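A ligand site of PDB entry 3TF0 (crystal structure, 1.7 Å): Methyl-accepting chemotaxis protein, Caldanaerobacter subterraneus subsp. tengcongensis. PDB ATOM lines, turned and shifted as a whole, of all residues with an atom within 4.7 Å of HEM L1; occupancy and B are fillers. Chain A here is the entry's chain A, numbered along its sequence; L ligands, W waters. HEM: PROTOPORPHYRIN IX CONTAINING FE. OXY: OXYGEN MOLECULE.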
ATOM      1  N   MET A   1      33.021 -18.669 -37.248  1.00  0.00           N
ATOM      2  CA  MET A   1      32.628 -17.974 -36.029  1.00  0.00           C
ATOM      3  C   MET A   1      33.604 -16.837 -35.762  1.00  0.00           C
ATOM      4  O   MET A   1      34.812 -17.014 -35.903  1.00  0.00           O
ATOM      5  CB  MET A   1      32.630 -18.938 -34.841  1.00  0.00           C
ATOM      6  CG  MET A   1      31.839 -18.460 -33.660  1.00  0.00           C
ATOM      7  SD  MET A   1      30.076 -18.332 -34.073  1.00  0.00           S
ATOM      8  CE  MET A   1      29.663 -20.078 -34.235  1.00  0.00           C
ATOM      9  N   LYS A   2      33.094 -15.687 -35.352  1.00  0.00           N
ATOM     10  CA  LYS A   2      33.989 -14.573 -35.065  1.00  0.00           C
ATOM     11  C   LYS A   2      35.053 -14.974 -34.037  1.00  0.00           C
ATOM     12  O   LYS A   2      34.753 -15.608 -33.013  1.00  0.00           O
ATOM     13  CB  LYS A   2      33.231 -13.353 -34.543  1.00  0.00           C
ATOM     14  CG  LYS A   2      34.133 -12.119 -34.467  1.00  0.00           C
ATOM     15  CD  LYS A   2      33.356 -10.828 -34.179  1.00  0.00           C
ATOM     16  CE  LYS A   2      34.297  -9.640 -34.301  1.00  0.00           C
ATOM     17  NZ  LYS A   2      33.712  -8.383 -33.726  1.00  0.00           N
ATOM     18  N   ILE A   5      34.778 -14.188 -30.186  1.00  0.00           N
ATOM     19  CA  ILE A   5      33.843 -15.043 -29.466  1.00  0.00           C
ATOM     20  C   ILE A   5      34.389 -16.446 -29.195  1.00  0.00           C
ATOM     21  O   ILE A   5      34.207 -17.011 -28.105  1.00  0.00           O
ATOM     22  CB  ILE A   5      32.502 -15.148 -30.184  1.00  0.00           C
ATOM     23  CG1 ILE A   5      31.976 -13.749 -30.557  1.00  0.00           C
ATOM     24  CG2 ILE A   5      31.504 -15.938 -29.357  1.00  0.00           C
ATOM     25  CD1 ILE A   5      31.770 -12.807 -29.364  1.00  0.00           C
ATOM     26  N   ILE A  75      28.191 -16.049 -20.308  1.00  0.00           N
ATOM     27  CA  ILE A  75      27.692 -14.728 -19.890  1.00  0.00           C
ATOM     28  C   ILE A  75      28.657 -14.094 -18.873  1.00  0.00           C
ATOM     29  O   ILE A  75      28.999 -12.905 -18.979  1.00  0.00           O
ATOM     30  CB  ILE A  75      26.273 -14.795 -19.284  1.00  0.00           C
ATOM     31  CG1 ILE A  75      25.226 -15.145 -20.375  1.00  0.00           C
ATOM     32  CG2 ILE A  75      25.915 -13.461 -18.622  1.00  0.00           C
ATOM     33  CD1 ILE A  75      25.222 -14.188 -21.534  1.00  0.00           C
ATOM     34  N   PHE A  78      31.686 -12.990 -20.865  1.00  0.00           N
ATOM     35  CA  PHE A  78      31.322 -11.749 -21.558  1.00  0.00           C
ATOM     36  C   PHE A  78      31.342 -10.545 -20.611  1.00  0.00           C
ATOM     37  O   PHE A  78      31.836  -9.471 -20.952  1.00  0.00           O
ATOM     38  CB  PHE A  78      29.927 -11.860 -22.162  1.00  0.00           C
ATOM     39  CG  PHE A  78      29.884 -12.595 -23.467  1.00  0.00           C
ATOM     40  CD1 PHE A  78      30.995 -12.662 -24.290  1.00  0.00           C
ATOM     41  CD2 PHE A  78      28.695 -13.190 -23.895  1.00  0.00           C
ATOM     42  CE1 PHE A  78      30.935 -13.320 -25.508  1.00  0.00           C
ATOM     43  CE2 PHE A  78      28.622 -13.852 -25.119  1.00  0.00           C
ATOM     44  CZ  PHE A  78      29.724 -13.910 -25.927  1.00  0.00           C
ATOM     45  N   PHE A  82      33.887  -7.977 -21.898  1.00  0.00           N
ATOM     46  CA  PHE A  82      33.195  -6.903 -22.604  1.00  0.00           C
ATOM     47  C   PHE A  82      32.147  -6.248 -21.704  1.00  0.00           C
ATOM     48  O   PHE A  82      30.949  -6.326 -21.966  1.00  0.00           O
ATOM     49  CB  PHE A  82      32.515  -7.462 -23.864  1.00  0.00           C
ATOM     50  CG  PHE A  82      33.364  -8.442 -24.634  1.00  0.00           C
ATOM     51  CD1 PHE A  82      34.653  -8.128 -25.021  1.00  0.00           C
ATOM     52  CD2 PHE A  82      32.861  -9.694 -24.974  1.00  0.00           C
ATOM     53  CE1 PHE A  82      35.428  -9.028 -25.725  1.00  0.00           C
ATOM     54  CE2 PHE A  82      33.622 -10.609 -25.690  1.00  0.00           C
ATOM     55  CZ  PHE A  82      34.909 -10.278 -26.063  1.00  0.00           C
ATOM     56  N   TYR A  85      28.762  -3.880 -22.382  1.00  0.00           N
ATOM     57  CA  TYR A  85      27.456  -4.370 -22.811  1.00  0.00           C
ATOM     58  C   TYR A  85      26.499  -4.661 -21.658  1.00  0.00           C
ATOM     59  O   TYR A  85      25.305  -4.865 -21.881  1.00  0.00           O
ATOM     60  CB  TYR A  85      27.589  -5.597 -23.707  1.00  0.00           C
ATOM     61  CG  TYR A  85      28.291  -5.305 -25.009  1.00  0.00           C
ATOM     62  CD1 TYR A  85      27.615  -4.689 -26.070  1.00  0.00           C
ATOM     63  CD2 TYR A  85      29.624  -5.638 -25.193  1.00  0.00           C
ATOM     64  CE1 TYR A  85      28.261  -4.415 -27.263  1.00  0.00           C
ATOM     65  CE2 TYR A  85      30.281  -5.373 -26.388  1.00  0.00           C
ATOM     66  CZ  TYR A  85      29.575  -4.754 -27.416  1.00  0.00           C
ATOM     67  OH  TYR A  85      30.210  -4.471 -28.608  1.00  0.00           O
ATOM     68  N   PHE A  86      27.019  -4.658 -20.432  1.00  0.00           N
ATOM     69  CA  PHE A  86      26.212  -4.973 -19.244  1.00  0.00           C
ATOM     70  C   PHE A  86      25.987  -3.718 -18.392  1.00  0.00           C
ATOM     71  O   PHE A  86      24.962  -3.587 -17.725  1.00  0.00           O
ATOM     72  CB  PHE A  86      26.895  -6.075 -18.422  1.00  0.00           C
ATOM     73  CG  PHE A  86      27.063  -7.373 -19.165  1.00  0.00           C
ATOM     74  CD1 PHE A  86      28.105  -7.536 -20.061  1.00  0.00           C
ATOM     75  CD2 PHE A  86      26.159  -8.418 -19.002  1.00  0.00           C
ATOM     76  CE1 PHE A  86      28.251  -8.708 -20.761  1.00  0.00           C
ATOM     77  CE2 PHE A  86      26.306  -9.602 -19.694  1.00  0.00           C
ATOM     78  CZ  PHE A  86      27.350  -9.754 -20.584  1.00  0.00           C
ATOM     79  N   PHE A  94      18.881  -5.605 -21.966  1.00  0.00           N
ATOM     80  CA  PHE A  94      19.976  -6.434 -22.461  1.00  0.00           C
ATOM     81  C   PHE A  94      19.490  -7.415 -23.539  1.00  0.00           C
ATOM     82  O   PHE A  94      20.020  -7.447 -24.644  1.00  0.00           O
ATOM     83  CB  PHE A  94      20.630  -7.184 -21.294  1.00  0.00           C
ATOM     84  CG  PHE A  94      21.803  -8.046 -21.685  1.00  0.00           C
ATOM     85  CD1 PHE A  94      23.068  -7.503 -21.844  1.00  0.00           C
ATOM     86  CD2 PHE A  94      21.642  -9.406 -21.878  1.00  0.00           C
ATOM     87  CE1 PHE A  94      24.144  -8.297 -22.202  1.00  0.00           C
ATOM     88  CE2 PHE A  94      22.712 -10.208 -22.234  1.00  0.00           C
ATOM     89  CZ  PHE A  94      23.960  -9.652 -22.399  1.00  0.00           C
ATOM     90  N   LEU A  95      18.460  -8.212 -23.221  1.00  0.00           N
ATOM     91  CA  LEU A  95      17.946  -9.149 -24.225  1.00  0.00           C
ATOM     92  C   LEU A  95      17.427  -8.454 -25.489  1.00  0.00           C
ATOM     93  O   LEU A  95      17.637  -8.939 -26.601  1.00  0.00           O
ATOM     94  CB  LEU A  95      16.861 -10.044 -23.632  1.00  0.00           C
ATOM     95  CG  LEU A  95      17.308 -10.927 -22.467  1.00  0.00           C
ATOM     96  CD1 LEU A  95      16.140 -11.619 -21.810  1.00  0.00           C
ATOM     97  CD2 LEU A  95      18.369 -11.953 -22.916  1.00  0.00           C
ATOM     98  N   MET A  98      20.132  -7.457 -28.154  1.00  0.00           N
ATOM     99  CA  MET A  98      21.025  -8.500 -28.665  1.00  0.00           C
ATOM    100  C   MET A  98      21.030  -8.610 -30.185  1.00  0.00           C
ATOM    101  O   MET A  98      22.091  -8.774 -30.784  1.00  0.00           O
ATOM    102  CB  MET A  98      20.741  -9.850 -28.012  1.00  0.00           C
ATOM    103  CG  MET A  98      21.290  -9.968 -26.566  1.00  0.00           C
ATOM    104  SD  MET A  98      23.090  -9.726 -26.417  1.00  0.00           S
ATOM    105  CE  MET A  98      23.201  -8.007 -25.946  1.00  0.00           C
ATOM    106  N   VAL A 101      23.197  -5.826 -31.508  1.00  0.00           N
ATOM    107  CA  VAL A 101      24.570  -6.031 -31.094  1.00  0.00           C
ATOM    108  C   VAL A 101      25.239  -7.030 -32.009  1.00  0.00           C
ATOM    109  O   VAL A 101      26.383  -6.824 -32.429  1.00  0.00           O
ATOM    110  CB  VAL A 101      24.673  -6.459 -29.619  1.00  0.00           C
ATOM    111  CG1 VAL A 101      26.062  -7.061 -29.297  1.00  0.00           C
ATOM    112  CG2 VAL A 101      24.358  -5.268 -28.717  1.00  0.00           C
ATOM    113  N   HIS A 102      24.537  -8.111 -32.346  1.00  0.00           N
ATOM    114  CA  HIS A 102      25.132  -9.144 -33.193  1.00  0.00           C
ATOM    115  C   HIS A 102      25.367  -8.697 -34.638  1.00  0.00           C
ATOM    116  O   HIS A 102      26.306  -9.153 -35.277  1.00  0.00           O
ATOM    117  CB  HIS A 102      24.377 -10.471 -33.101  1.00  0.00           C
ATOM    118  CG  HIS A 102      24.585 -11.184 -31.799  1.00  0.00           C
ATOM    119  ND1 HIS A 102      24.059 -10.708 -30.606  1.00  0.00           N
ATOM    120  CD2 HIS A 102      25.276 -12.300 -31.485  1.00  0.00           C
ATOM    121  CE1 HIS A 102      24.419 -11.522 -29.623  1.00  0.00           C
ATOM    122  NE2 HIS A 102      25.155 -12.491 -30.127  1.00  0.00           N
ATOM    123  N   LEU A 105      28.479  -6.238 -34.318  1.00  0.00           N
ATOM    124  CA  LEU A 105      29.771  -6.861 -34.053  1.00  0.00           C
ATOM    125  C   LEU A 105      30.231  -7.729 -35.220  1.00  0.00           C
ATOM    126  O   LEU A 105      31.350  -8.223 -35.197  1.00  0.00           O
ATOM    127  CB  LEU A 105      29.745  -7.672 -32.750  1.00  0.00           C
ATOM    128  CG  LEU A 105      29.624  -6.815 -31.496  1.00  0.00           C
ATOM    129  CD1 LEU A 105      29.547  -7.670 -30.249  1.00  0.00           C
ATOM    130  CD2 LEU A 105      30.803  -5.838 -31.418  1.00  0.00           C
ATOM    131  N   THR A 106      29.374  -7.924 -36.228  1.00  0.00           N
ATOM    132  CA  THR A 106      29.793  -8.708 -37.391  1.00  0.00           C
ATOM    133  C   THR A 106      29.772  -7.899 -38.694  1.00  0.00           C
ATOM    134  O   THR A 106      30.062  -8.427 -39.759  1.00  0.00           O
ATOM    135  CB  THR A 106      28.990 -10.008 -37.565  1.00  0.00           C
ATOM    136  OG1 THR A 106      27.593  -9.707 -37.700  1.00  0.00           O
ATOM    137  CG2 THR A 106      29.204 -10.946 -36.372  1.00  0.00           C
ATOM    138  N   THR A 113      27.309 -13.895 -41.187  1.00  0.00           N
ATOM    139  CA  THR A 113      26.034 -14.568 -40.994  1.00  0.00           C
ATOM    140  C   THR A 113      25.725 -14.641 -39.489  1.00  0.00           C
ATOM    141  O   THR A 113      25.677 -15.729 -38.920  1.00  0.00           O
ATOM    142  CB  THR A 113      26.081 -15.999 -41.544  1.00  0.00           C
ATOM    143  OG1 THR A 113      27.188 -16.699 -40.950  1.00  0.00           O
ATOM    144  CG2 THR A 113      26.263 -15.993 -43.057  1.00  0.00           C
ATOM    145  N   PRO A 114      25.541 -13.473 -38.848  1.00  0.00           N
ATOM    146  CA  PRO A 114      25.257 -13.538 -37.412  1.00  0.00           C
ATOM    147  C   PRO A 114      23.916 -14.213 -37.152  1.00  0.00           C
ATOM    148  O   PRO A 114      23.075 -14.249 -38.038  1.00  0.00           O
ATOM    149  CB  PRO A 114      25.179 -12.052 -37.016  1.00  0.00           C
ATOM    150  CG  PRO A 114      24.828 -11.338 -38.298  1.00  0.00           C
ATOM    151  CD  PRO A 114      25.542 -12.099 -39.368  1.00  0.00           C
ATOM    152  N   PRO A 115      23.726 -14.740 -35.933  1.00  0.00           N
ATOM    153  CA  PRO A 115      22.389 -15.229 -35.600  1.00  0.00           C
ATOM    154  C   PRO A 115      21.476 -14.034 -35.490  1.00  0.00           C
ATOM    155  O   PRO A 115      21.952 -12.953 -35.142  1.00  0.00           O
ATOM    156  CB  PRO A 115      22.563 -15.828 -34.217  1.00  0.00           C
ATOM    157  CG  PRO A 115      23.797 -15.090 -33.612  1.00  0.00           C
ATOM    158  CD  PRO A 115      24.677 -14.809 -34.804  1.00  0.00           C
ATOM    159  N   LEU A 117      18.179 -12.523 -33.430  1.00  0.00           N
ATOM    160  CA  LEU A 117      17.732 -12.737 -32.053  1.00  0.00           C
ATOM    161  C   LEU A 117      16.622 -11.741 -31.731  1.00  0.00           C
ATOM    162  O   LEU A 117      16.574 -11.179 -30.623  1.00  0.00           O
ATOM    163  CB  LEU A 117      18.909 -12.533 -31.098  1.00  0.00           C
ATOM    164  CG  LEU A 117      20.128 -13.414 -31.359  1.00  0.00           C
ATOM    165  CD1 LEU A 117      21.386 -12.827 -30.690  1.00  0.00           C
ATOM    166  CD2 LEU A 117      19.890 -14.838 -30.883  1.00  0.00           C
ATOM    167  N   MET A 129      11.277 -14.117 -27.959  1.00  0.00           N
ATOM    168  CA  MET A 129      12.560 -13.951 -28.612  1.00  0.00           C
ATOM    169  C   MET A 129      12.732 -15.123 -29.544  1.00  0.00           C
ATOM    170  O   MET A 129      12.442 -16.265 -29.175  1.00  0.00           O
ATOM    171  CB  MET A 129      13.680 -13.909 -27.581  1.00  0.00           C
ATOM    172  CG  MET A 129      15.028 -13.480 -28.093  1.00  0.00           C
ATOM    173  SD  MET A 129      16.139 -13.176 -26.703  1.00  0.00           S
ATOM    174  CE  MET A 129      17.631 -12.634 -27.524  1.00  0.00           C
ATOM    175  N   TYR A 131      15.406 -17.144 -31.988  1.00  0.00           N
ATOM    176  CA  TYR A 131      16.723 -17.433 -32.507  1.00  0.00           C
ATOM    177  C   TYR A 131      16.573 -17.921 -33.931  1.00  0.00           C
ATOM    178  O   TYR A 131      15.814 -18.858 -34.192  1.00  0.00           O
ATOM    179  CB  TYR A 131      17.330 -18.565 -31.673  1.00  0.00           C
ATOM    180  CG  TYR A 131      18.561 -19.208 -32.278  1.00  0.00           C
ATOM    181  CD1 TYR A 131      19.801 -18.586 -32.201  1.00  0.00           C
ATOM    182  CD2 TYR A 131      18.489 -20.444 -32.924  1.00  0.00           C
ATOM    183  CE1 TYR A 131      20.934 -19.180 -32.735  1.00  0.00           C
ATOM    184  CE2 TYR A 131      19.621 -21.051 -33.465  1.00  0.00           C
ATOM    185  CZ  TYR A 131      20.836 -20.406 -33.363  1.00  0.00           C
ATOM    186  OH  TYR A 131      21.951 -20.988 -33.902  1.00  0.00           O
ATOM    187  N   SER A 133      19.145 -18.947 -37.264  1.00  0.00           N
ATOM    188  CA  SER A 133      20.503 -19.086 -37.756  1.00  0.00           C
ATOM    189  C   SER A 133      20.662 -20.360 -38.570  1.00  0.00           C
ATOM    190  O   SER A 133      19.991 -21.347 -38.320  1.00  0.00           O
ATOM    191  CB  SER A 133      21.483 -19.105 -36.575  1.00  0.00           C
ATOM    192  OG  SER A 133      22.810 -19.351 -36.996  1.00  0.00           O
ATOM    193  N   ARG A 135      23.139 -22.104 -38.091  1.00  0.00           N
ATOM    194  CA  ARG A 135      24.074 -22.894 -37.270  1.00  0.00           C
ATOM    195  C   ARG A 135      23.490 -23.910 -36.275  1.00  0.00           C
ATOM    196  O   ARG A 135      24.227 -24.763 -35.753  1.00  0.00           O
ATOM    197  CB  ARG A 135      25.063 -21.983 -36.535  1.00  0.00           C
ATOM    198  CG  ARG A 135      25.938 -21.131 -37.432  1.00  0.00           C
ATOM    199  CD  ARG A 135      27.097 -20.575 -36.619  1.00  0.00           C
ATOM    200  NE  ARG A 135      27.991 -19.750 -37.411  1.00  0.00           N
ATOM    201  CZ  ARG A 135      27.933 -18.419 -37.471  1.00  0.00           C
ATOM    202  NH1 ARG A 135      27.006 -17.761 -36.789  1.00  0.00           N
ATOM    203  NH2 ARG A 135      28.800 -17.758 -38.220  1.00  0.00           N
ATOM    204  N   MET A 137      22.465 -23.756 -33.123  1.00  0.00           N
ATOM    205  CA  MET A 137      23.074 -23.746 -31.810  1.00  0.00           C
ATOM    206  C   MET A 137      22.048 -23.479 -30.718  1.00  0.00           C
ATOM    207  O   MET A 137      22.162 -22.540 -29.936  1.00  0.00           O
ATOM    208  CB  MET A 137      24.233 -22.750 -31.794  1.00  0.00           C
ATOM    209  CG  MET A 137      25.366 -23.205 -32.711  1.00  0.00           C
ATOM    210  SD  MET A 137      26.730 -22.046 -32.764  1.00  0.00           S
ATOM    211  CE  MET A 137      27.368 -22.239 -31.079  1.00  0.00           C
ATOM    212  N   TYR A 140      23.226 -23.553 -26.848  1.00  0.00           N
ATOM    213  CA  TYR A 140      24.014 -22.356 -26.570  1.00  0.00           C
ATOM    214  C   TYR A 140      23.098 -21.129 -26.339  1.00  0.00           C
ATOM    215  O   TYR A 140      23.236 -20.433 -25.333  1.00  0.00           O
ATOM    216  CB  TYR A 140      25.013 -22.096 -27.706  1.00  0.00           C
ATOM    217  CG  TYR A 140      25.941 -20.930 -27.418  1.00  0.00           C
ATOM    218  CD1 TYR A 140      26.719 -20.923 -26.266  1.00  0.00           C
ATOM    219  CD2 TYR A 140      26.029 -19.855 -28.308  1.00  0.00           C
ATOM    220  CE1 TYR A 140      27.593 -19.870 -25.981  1.00  0.00           C
ATOM    221  CE2 TYR A 140      26.889 -18.794 -28.050  1.00  0.00           C
ATOM    222  CZ  TYR A 140      27.646 -18.793 -26.880  1.00  0.00           C
ATOM    223  OH  TYR A 140      28.499 -17.751 -26.614  1.00  0.00           O
ATOM    224  N   PHE A 141      22.144 -20.914 -27.257  1.00  0.00           N
ATOM    225  CA  PHE A 141      21.160 -19.830 -27.149  1.00  0.00           C
ATOM    226  C   PHE A 141      20.415 -19.918 -25.825  1.00  0.00           C
ATOM    227  O   PHE A 141      20.345 -18.929 -25.089  1.00  0.00           O
ATOM    228  CB  PHE A 141      20.206 -19.923 -28.353  1.00  0.00           C
ATOM    229  CG  PHE A 141      18.980 -19.047 -28.262  1.00  0.00           C
ATOM    230  CD1 PHE A 141      19.070 -17.666 -28.409  1.00  0.00           C
ATOM    231  CD2 PHE A 141      17.728 -19.623 -28.075  1.00  0.00           C
ATOM    232  CE1 PHE A 141      17.911 -16.873 -28.347  1.00  0.00           C
ATOM    233  CE2 PHE A 141      16.580 -18.851 -28.007  1.00  0.00           C
ATOM    234  CZ  PHE A 141      16.671 -17.482 -28.146  1.00  0.00           C
ATOM    235  N   LEU A 144      22.698 -19.111 -22.815  1.00  0.00           N
ATOM    236  CA  LEU A 144      22.995 -17.687 -22.671  1.00  0.00           C
ATOM    237  C   LEU A 144      21.825 -16.955 -22.006  1.00  0.00           C
ATOM    238  O   LEU A 144      22.008 -16.032 -21.226  1.00  0.00           O
ATOM    239  CB  LEU A 144      23.305 -17.069 -24.031  1.00  0.00           C
ATOM    240  CG  LEU A 144      24.644 -17.494 -24.664  1.00  0.00           C
ATOM    241  CD1 LEU A 144      24.635 -17.140 -26.144  1.00  0.00           C
ATOM    242  CD2 LEU A 144      25.844 -16.834 -23.981  1.00  0.00           C
ATOM    243  N   ILE A 145      20.617 -17.390 -22.307  1.00  0.00           N
ATOM    244  CA  ILE A 145      19.448 -16.747 -21.718  1.00  0.00           C
ATOM    245  C   ILE A 145      19.444 -17.038 -20.231  1.00  0.00           C
ATOM    246  O   ILE A 145      19.246 -16.141 -19.410  1.00  0.00           O
ATOM    247  CB  ILE A 145      18.130 -17.195 -22.375  1.00  0.00           C
ATOM    248  CG1 ILE A 145      18.094 -16.741 -23.839  1.00  0.00           C
ATOM    249  CG2 ILE A 145      16.919 -16.682 -21.577  1.00  0.00           C
ATOM    250  CD1 ILE A 145      16.861 -17.205 -24.593  1.00  0.00           C
ATOM    251  N   SER A 148      22.172 -15.088 -18.464  1.00  0.00           N
ATOM    252  CA  SER A 148      21.818 -13.677 -18.419  1.00  0.00           C
ATOM    253  C   SER A 148      20.932 -13.413 -17.204  1.00  0.00           C
ATOM    254  O   SER A 148      21.147 -12.456 -16.465  1.00  0.00           O
ATOM    255  CB  SER A 148      21.132 -13.264 -19.716  1.00  0.00           C
ATOM    256  OG  SER A 148      22.036 -13.332 -20.803  1.00  0.00           O
HETATM  257  CHA HEM L   1      27.426 -15.796 -31.467  1.00  0.00           C
HETATM  258  CHB HEM L   1      28.509 -11.500 -29.505  1.00  0.00           C
HETATM  259  CHC HEM L   1      25.367 -12.387 -25.937  1.00  0.00           C
HETATM  260  CHD HEM L   1      23.275 -15.551 -28.888  1.00  0.00           C
HETATM  261  C1A HEM L   1      27.987 -14.560 -31.278  1.00  0.00           C
HETATM  262  C2A HEM L   1      28.932 -13.887 -32.145  1.00  0.00           C
HETATM  263  C3A HEM L   1      29.213 -12.703 -31.607  1.00  0.00           C
HETATM  264  C4A HEM L   1      28.468 -12.573 -30.374  1.00  0.00           C
HETATM  265  CMA HEM L   1      30.179 -11.638 -32.201  1.00  0.00           C
HETATM  266  CAA HEM L   1      29.527 -14.437 -33.475  1.00  0.00           C
HETATM  267  CBA HEM L   1      28.508 -14.443 -34.600  1.00  0.00           C
HETATM  268  CGA HEM L   1      29.130 -14.883 -35.915  1.00  0.00           C
HETATM  269  O1A HEM L   1      28.371 -15.074 -36.894  1.00  0.00           O
HETATM  270  O2A HEM L   1      30.379 -15.049 -36.012  1.00  0.00           O
HETATM  271  C1B HEM L   1      27.851 -11.417 -28.298  1.00  0.00           C
HETATM  272  C2B HEM L   1      28.139 -10.505 -27.190  1.00  0.00           C
HETATM  273  C3B HEM L   1      27.259 -10.765 -26.206  1.00  0.00           C
HETATM  274  C4B HEM L   1      26.400 -11.841 -26.663  1.00  0.00           C
HETATM  275  CMB HEM L   1      29.258  -9.442 -27.198  1.00  0.00           C
HETATM  276  CAB HEM L   1      27.086 -10.093 -24.833  1.00  0.00           C
HETATM  277  CBB HEM L   1      27.775  -8.999 -24.473  1.00  0.00           C
HETATM  278  C1C HEM L   1      24.437 -13.218 -26.504  1.00  0.00           C
HETATM  279  C2C HEM L   1      23.113 -13.502 -25.999  1.00  0.00           C
HETATM  280  C3C HEM L   1      22.527 -14.372 -26.837  1.00  0.00           C
HETATM  281  C4C HEM L   1      23.470 -14.658 -27.887  1.00  0.00           C
HETATM  282  CMC HEM L   1      22.516 -12.891 -24.706  1.00  0.00           C
HETATM  283  CAC HEM L   1      21.136 -15.022 -26.777  1.00  0.00           C
HETATM  284  CBC HEM L   1      20.196 -14.588 -25.931  1.00  0.00           C
HETATM  285  C1D HEM L   1      24.275 -16.077 -29.684  1.00  0.00           C
HETATM  286  C2D HEM L   1      24.282 -17.382 -30.282  1.00  0.00           C
HETATM  287  C3D HEM L   1      25.569 -17.458 -31.101  1.00  0.00           C
HETATM  288  C4D HEM L   1      26.220 -16.178 -30.912  1.00  0.00           C
HETATM  289  CMD HEM L   1      23.197 -18.468 -30.149  1.00  0.00           C
HETATM  290  CAD HEM L   1      26.073 -18.662 -31.938  1.00  0.00           C
HETATM  291  CBD HEM L   1      26.099 -18.323 -33.415  1.00  0.00           C
HETATM  292  CGD HEM L   1      24.876 -18.863 -34.104  1.00  0.00           C
HETATM  293  O1D HEM L   1      24.076 -19.592 -33.471  1.00  0.00           O
HETATM  294  O2D HEM L   1      24.698 -18.569 -35.308  1.00  0.00           O
HETATM  295  NA  HEM L   1      27.711 -13.721 -30.208  1.00  0.00           N
HETATM  296  NB  HEM L   1      26.800 -12.227 -27.919  1.00  0.00           N
HETATM  297  NC  HEM L   1      24.627 -13.937 -27.657  1.00  0.00           N
HETATM  298  ND  HEM L   1      25.434 -15.417 -30.067  1.00  0.00           N
HETATM  299 FE   HEM L   1      26.178 -13.862 -28.933  1.00  0.00          FE
HETATM  300  O1  OXY L   2      27.007 -15.015 -27.645  1.00  0.00           O
HETATM  301  O2  OXY L   2      28.121 -15.855 -28.578  1.00  0.00           O
HETATM  302  O   HOH W   1      31.305 -16.076 -38.272  1.00  0.00           O
HETATM  303  O   HOH W   2      29.460 -14.190 -39.210  1.00  0.00           O
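O1 of OXY L2 binds FE of HEM L1, 1.9 Å away.
The guanidinium group of Arg 135 is in salt-bridge range of an oxygen (O2D) of HEM L1, at 2.9 Å. The side-chain hydroxyl (OH) of Tyr 131 is in hydrogen-bond range of an oxygen (O1D) of HEM L1 (2.6 Å). An oxygen (O2) of OXY L2 sits at hydrogen-bond distance from the side-chain hydroxyl (OH) of Tyr 140, at 2.8 Å. The backbone NH (N) of Lys 2 sits at hydrogen-bond distance from an oxygen (O2A) of HEM L1, 2.9 Å away. FE of HEM L1 is bound by NE2 of His 102 (2.1 Å). The side-chain hydroxyl (OG) of Ser 133 is in hydrogen-bond range of an oxygen (O2D) of HEM L1 (2.7 Å).
NZ of Lys 2 is in hydrogen-bond range of O of Leu 105 (2.8 Å). The backbone carbonyl oxygen (O) of Leu 144 lies within hydrogen-bond range of the side-chain hydroxyl (OG) of Ser 148, 2.7 Å away. The backbone NH (N) of Arg 135 is in hydrogen-bond range of the side-chain hydroxyl (OG) of Ser 133 (3.0 Å). NH1 of Arg 135 lies within hydrogen-bond range of O of Thr 113. O of His 102 lies within hydrogen-bond range of OG1 of Thr 106 (2.8 Å). OH of Tyr 131 lies within hydrogen-bond range of N of Met 137 (2.9 Å). A ring nitrogen (ND1) of His 102 is in hydrogen-bond range of the backbone carbonyl oxygen (O) of Met 98, at 2.8 Å.
Water W2 bridges O1A of HEM L1 (2.7 Å) and N of Thr 113 (2.9 Å).
An oxygen (O1A) of HEM L1 sits close to the backbone carbonyl oxygen (O) of Thr 113 (3.4 Å). SD of Met 137 lies close to O1D of HEM L1 (3.7 Å). Residues that only touch HEM L1: Met 1 (3.7 Å), Ile 5 (3.1 Å), Phe 78 (3.4 Å), Tyr 85 (3.5 Å), Phe 86 (3.8 Å), Phe 94 (3.7 Å), Met 98 (3.5 Å), Leu 105 (3.5 Å), Thr 106 (3.96 Å), Pro 114 (3.5 Å), Pro 115 (3.6 Å), Leu 117 (3.8 Å), Met 129 (3.6 Å), Tyr 140 (3.6 Å), Phe 141 (3.7 Å), Leu 144 (3.2 Å), Ile 145 (3.7 Å) and Ser 148 (3.96 Å). Within 4 Å of HEM L1: Met 1, Lys 2, Ile 5, Phe 78, Tyr 85, Phe 86, Phe 94, Met 98, His 102, Leu 105, Thr 106, Thr 113, Pro 114, Pro 115, Leu 117, Met 129, Tyr 131, Ser 133, Arg 135, Met 137, Tyr 140, Phe 141, Leu 144, Ile 145 and Ser 148. The nearest printed residue that does not touch HEM L1 is Phe 82 (4.2 Å).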
